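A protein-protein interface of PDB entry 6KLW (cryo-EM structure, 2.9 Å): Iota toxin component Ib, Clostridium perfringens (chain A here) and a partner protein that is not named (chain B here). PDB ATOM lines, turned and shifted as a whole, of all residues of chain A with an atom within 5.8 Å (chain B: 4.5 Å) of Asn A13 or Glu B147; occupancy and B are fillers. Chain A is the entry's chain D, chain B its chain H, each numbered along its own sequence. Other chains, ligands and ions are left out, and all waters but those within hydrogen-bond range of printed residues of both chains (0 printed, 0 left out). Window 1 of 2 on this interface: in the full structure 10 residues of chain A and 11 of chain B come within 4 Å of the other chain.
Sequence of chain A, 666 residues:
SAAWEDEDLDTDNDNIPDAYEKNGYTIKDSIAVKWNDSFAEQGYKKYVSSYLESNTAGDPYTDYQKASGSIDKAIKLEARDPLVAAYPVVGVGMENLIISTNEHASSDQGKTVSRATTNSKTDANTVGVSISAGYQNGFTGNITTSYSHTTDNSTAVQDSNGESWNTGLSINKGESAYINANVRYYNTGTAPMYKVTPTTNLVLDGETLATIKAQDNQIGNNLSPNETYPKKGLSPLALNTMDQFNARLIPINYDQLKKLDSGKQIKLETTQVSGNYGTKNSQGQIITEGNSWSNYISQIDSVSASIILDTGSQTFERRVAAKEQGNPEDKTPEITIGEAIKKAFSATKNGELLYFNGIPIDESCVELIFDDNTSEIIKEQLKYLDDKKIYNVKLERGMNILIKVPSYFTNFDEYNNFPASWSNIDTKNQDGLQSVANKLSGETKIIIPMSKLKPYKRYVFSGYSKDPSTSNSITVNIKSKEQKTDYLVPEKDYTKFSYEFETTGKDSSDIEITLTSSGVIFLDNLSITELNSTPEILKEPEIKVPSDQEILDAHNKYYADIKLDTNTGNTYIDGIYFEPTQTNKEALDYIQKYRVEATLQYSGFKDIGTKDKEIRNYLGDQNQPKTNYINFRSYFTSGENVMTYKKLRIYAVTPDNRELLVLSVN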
ATOM      1  N   ASP A  10      -3.987  17.123  -3.123  1.00  0.00           N
ATOM      2  CA  ASP A  10      -4.367  18.347  -2.421  1.00  0.00           C
ATOM      3  C   ASP A  10      -3.366  18.581  -1.293  1.00  0.00           C
ATOM      4  O   ASP A  10      -3.535  18.059  -0.190  1.00  0.00           O
ATOM      5  CB  ASP A  10      -5.793  18.226  -1.897  1.00  0.00           C
ATOM      6  CG  ASP A  10      -6.311  19.507  -1.291  1.00  0.00           C
ATOM      7  OD1 ASP A  10      -5.774  20.588  -1.609  1.00  0.00           O
ATOM      8  OD2 ASP A  10      -7.273  19.432  -0.503  1.00  0.00           O
ATOM      9  N   THR A  11      -2.331  19.376  -1.561  1.00  0.00           N
ATOM     10  CA  THR A  11      -1.224  19.492  -0.618  1.00  0.00           C
ATOM     11  C   THR A  11      -1.644  20.202   0.665  1.00  0.00           C
ATOM     12  O   THR A  11      -1.395  19.707   1.768  1.00  0.00           O
ATOM     13  CB  THR A  11      -0.053  20.216  -1.277  1.00  0.00           C
ATOM     14  OG1 THR A  11       0.384  19.474  -2.422  1.00  0.00           O
ATOM     15  CG2 THR A  11       1.097  20.339  -0.312  1.00  0.00           C
ATOM     16  N   ASP A  12      -2.276  21.366   0.547  1.00  0.00           N
ATOM     17  CA  ASP A  12      -2.702  22.118   1.721  1.00  0.00           C
ATOM     18  C   ASP A  12      -3.921  21.517   2.406  1.00  0.00           C
ATOM     19  O   ASP A  12      -4.260  21.952   3.511  1.00  0.00           O
ATOM     20  CB  ASP A  12      -2.989  23.571   1.343  1.00  0.00           C
ATOM     21  CG  ASP A  12      -3.954  23.692   0.197  1.00  0.00           C
ATOM     22  OD1 ASP A  12      -4.411  22.652  -0.307  1.00  0.00           O
ATOM     23  OD2 ASP A  12      -4.261  24.832  -0.204  1.00  0.00           O
ATOM     24  N   ASN A  13      -4.580  20.539   1.783  1.00  0.00           N
ATOM     25  CA  ASN A  13      -5.728  19.841   2.361  1.00  0.00           C
ATOM     26  C   ASN A  13      -6.874  20.807   2.673  1.00  0.00           C
ATOM     27  O   ASN A  13      -7.243  21.030   3.825  1.00  0.00           O
ATOM     28  CB  ASN A  13      -5.315  19.055   3.610  1.00  0.00           C
ATOM     29  CG  ASN A  13      -6.436  18.199   4.159  1.00  0.00           C
ATOM     30  OD1 ASN A  13      -7.375  17.852   3.446  1.00  0.00           O
ATOM     31  ND2 ASN A  13      -6.344  17.854   5.434  1.00  0.00           N
ATOM     32  N   ASP A  14      -7.432  21.390   1.614  1.00  0.00           N
ATOM     33  CA  ASP A  14      -8.599  22.252   1.747  1.00  0.00           C
ATOM     34  C   ASP A  14      -9.634  21.999   0.656  1.00  0.00           C
ATOM     35  O   ASP A  14     -10.418  22.895   0.338  1.00  0.00           O
ATOM     36  CB  ASP A  14      -8.184  23.723   1.769  1.00  0.00           C
ATOM     37  CG  ASP A  14      -7.737  24.225   0.425  1.00  0.00           C
ATOM     38  OD1 ASP A  14      -7.051  23.483  -0.297  1.00  0.00           O
ATOM     39  OD2 ASP A  14      -8.059  25.379   0.095  1.00  0.00           O
ATOM     40  N   ASN A  15      -9.644  20.799   0.079  1.00  0.00           N
ATOM     41  CA  ASN A  15     -10.662  20.300  -0.844  1.00  0.00           C
ATOM     42  C   ASN A  15     -10.587  20.923  -2.230  1.00  0.00           C
ATOM     43  O   ASN A  15     -11.536  20.793  -3.009  1.00  0.00           O
ATOM     44  CB  ASN A  15     -12.080  20.477  -0.286  1.00  0.00           C
ATOM     45  CG  ASN A  15     -12.238  19.894   1.092  1.00  0.00           C
ATOM     46  OD1 ASN A  15     -11.559  18.935   1.459  1.00  0.00           O
ATOM     47  ND2 ASN A  15     -13.141  20.469   1.872  1.00  0.00           N
ATOM     48  N   SER A  54      -3.652  27.142   3.181  1.00  0.00           N
ATOM     49  CA  SER A  54      -5.067  26.834   3.343  1.00  0.00           C
ATOM     50  C   SER A  54      -5.897  28.110   3.392  1.00  0.00           C
ATOM     51  O   SER A  54      -6.961  28.191   2.775  1.00  0.00           O
ATOM     52  CB  SER A  54      -5.276  26.004   4.604  1.00  0.00           C
ATOM     53  OG  SER A  54      -6.645  25.720   4.794  1.00  0.00           O
ATOM     54  N   TYR B  96     -13.675  11.416  11.112  1.00  0.00           N
ATOM     55  CA  TYR B  96     -12.331  11.214  10.591  1.00  0.00           C
ATOM     56  C   TYR B  96     -11.613  10.194  11.460  1.00  0.00           C
ATOM     57  O   TYR B  96     -11.662  10.285  12.690  1.00  0.00           O
ATOM     58  CB  TYR B  96     -11.536  12.528  10.577  1.00  0.00           C
ATOM     59  CG  TYR B  96     -12.271  13.707   9.974  1.00  0.00           C
ATOM     60  CD1 TYR B  96     -13.196  14.431  10.717  1.00  0.00           C
ATOM     61  CD2 TYR B  96     -12.025  14.111   8.670  1.00  0.00           C
ATOM     62  CE1 TYR B  96     -13.867  15.508  10.169  1.00  0.00           C
ATOM     63  CE2 TYR B  96     -12.679  15.192   8.120  1.00  0.00           C
ATOM     64  CZ  TYR B  96     -13.605  15.881   8.868  1.00  0.00           C
ATOM     65  OH  TYR B  96     -14.258  16.957   8.311  1.00  0.00           O
ATOM     66  N   TYR B 146     -13.136  16.034  13.791  1.00  0.00           N
ATOM     67  CA  TYR B 146     -12.280  16.993  13.106  1.00  0.00           C
ATOM     68  C   TYR B 146     -11.002  16.299  12.662  1.00  0.00           C
ATOM     69  O   TYR B 146     -10.519  15.396  13.349  1.00  0.00           O
ATOM     70  CB  TYR B 146     -11.943  18.181  14.011  1.00  0.00           C
ATOM     71  CG  TYR B 146     -13.147  18.984  14.441  1.00  0.00           C
ATOM     72  CD1 TYR B 146     -13.763  19.866  13.566  1.00  0.00           C
ATOM     73  CD2 TYR B 146     -13.667  18.861  15.721  1.00  0.00           C
ATOM     74  CE1 TYR B 146     -14.862  20.602  13.952  1.00  0.00           C
ATOM     75  CE2 TYR B 146     -14.768  19.594  16.117  1.00  0.00           C
ATOM     76  CZ  TYR B 146     -15.361  20.463  15.227  1.00  0.00           C
ATOM     77  OH  TYR B 146     -16.457  21.199  15.610  1.00  0.00           O
ATOM     78  N   GLU B 147     -10.455  16.734  11.524  1.00  0.00           N
ATOM     79  CA  GLU B 147      -9.233  16.158  10.986  1.00  0.00           C
ATOM     80  C   GLU B 147      -8.105  16.220  12.013  1.00  0.00           C
ATOM     81  O   GLU B 147      -8.139  17.034  12.941  1.00  0.00           O
ATOM     82  CB  GLU B 147      -8.820  16.900   9.716  1.00  0.00           C
ATOM     83  CG  GLU B 147      -9.981  17.297   8.835  1.00  0.00           C
ATOM     84  CD  GLU B 147      -9.553  17.677   7.433  1.00  0.00           C
ATOM     85  OE1 GLU B 147     -10.337  18.363   6.745  1.00  0.00           O
ATOM     86  OE2 GLU B 147      -8.441  17.289   7.016  1.00  0.00           O
ATOM     87  N   PRO B 148      -7.090  15.367  11.869  1.00  0.00           N
ATOM     88  CA  PRO B 148      -5.960  15.409  12.802  1.00  0.00           C
ATOM     89  C   PRO B 148      -5.159  16.691  12.649  1.00  0.00           C
ATOM     90  O   PRO B 148      -5.025  17.242  11.554  1.00  0.00           O
ATOM     91  CB  PRO B 148      -5.129  14.185  12.407  1.00  0.00           C
ATOM     92  CG  PRO B 148      -5.453  13.983  10.972  1.00  0.00           C
ATOM     93  CD  PRO B 148      -6.916  14.305  10.863  1.00  0.00           C
ATOM     94  N   GLY B 149      -4.619  17.160  13.769  1.00  0.00           N
ATOM     95  CA  GLY B 149      -3.787  18.346  13.772  1.00  0.00           C
ATOM     96  C   GLY B 149      -2.412  18.084  14.343  1.00  0.00           C
ATOM     97  O   GLY B 149      -1.788  17.066  14.032  1.00  0.00           O
ATOM     98  N   ILE B 197      -2.142  13.805   0.744  1.00  0.00           N
ATOM     99  CA  ILE B 197      -2.215  15.010   1.558  1.00  0.00           C
ATOM    100  C   ILE B 197      -0.865  15.217   2.223  1.00  0.00           C
ATOM    101  O   ILE B 197      -0.142  14.256   2.499  1.00  0.00           O
ATOM    102  CB  ILE B 197      -3.333  14.885   2.621  1.00  0.00           C
ATOM    103  CG1 ILE B 197      -4.693  14.680   1.967  1.00  0.00           C
ATOM    104  CG2 ILE B 197      -3.389  16.102   3.515  1.00  0.00           C
ATOM    105  CD1 ILE B 197      -5.174  15.860   1.188  1.00  0.00           C
ATOM    106  N   LYS B 206      -5.815  10.850   2.147  1.00  0.00           N
ATOM    107  CA  LYS B 206      -7.186  11.134   2.550  1.00  0.00           C
ATOM    108  C   LYS B 206      -8.129  10.461   1.562  1.00  0.00           C
ATOM    109  O   LYS B 206      -8.152  10.815   0.378  1.00  0.00           O
ATOM    110  CB  LYS B 206      -7.457  12.635   2.609  1.00  0.00           C
ATOM    111  CG  LYS B 206      -8.705  12.997   3.392  1.00  0.00           C
ATOM    112  CD  LYS B 206      -8.892  14.497   3.489  1.00  0.00           C
ATOM    113  CE  LYS B 206     -10.235  14.834   4.110  1.00  0.00           C
ATOM    114  NZ  LYS B 206     -11.358  14.168   3.391  1.00  0.00           N
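The side-chain carboxylate (OE2) of Glu B147 lies within hydrogen-bond range of the side-chain amide nitrogen (ND2) of Asn A13, 2.7 Å away.
OD2 of Asp A10 sits at hydrogen-bond distance from N of Asn A15.
Among the printed residues, merely in contact across the chains: Asp A10 with Ile B197 (3.1 Å), Asn A13 with Ile B197 (3.5 Å) and Asn A13 with Lys B206 (3.7 Å).
Of the printed residues of chain B, Asp A10 touches Ile B197. Asp A12 touches none of the printed residues of chain B. Asn A13 touches three residues of chain B. Of chain A, only Asn A13 (2.7 Å) comes within 4 Å of Glu B147. Pro B148 touches none of the printed residues of chain A. Of the printed residues of chain A, Ile B197 touches Asp A10 and Asn A13. Of the printed residues of chain A, Lys B206 touches Asn A13. The nearest printed residue of chain B that does not touch Asn A13 is Pro B148 (6.3 Å).
Hydrophobic or aromatic side chains of chain B within 4 Å of the printed part of chain A: Ile B197. Along chain B the printed residues that touch a printed residue of chain A span positions 147 to 206. Of the 7 printed residues of chain A, 2 touch a printed residue of chain B. Among the printed residues, 4 pairs touch across the chains.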
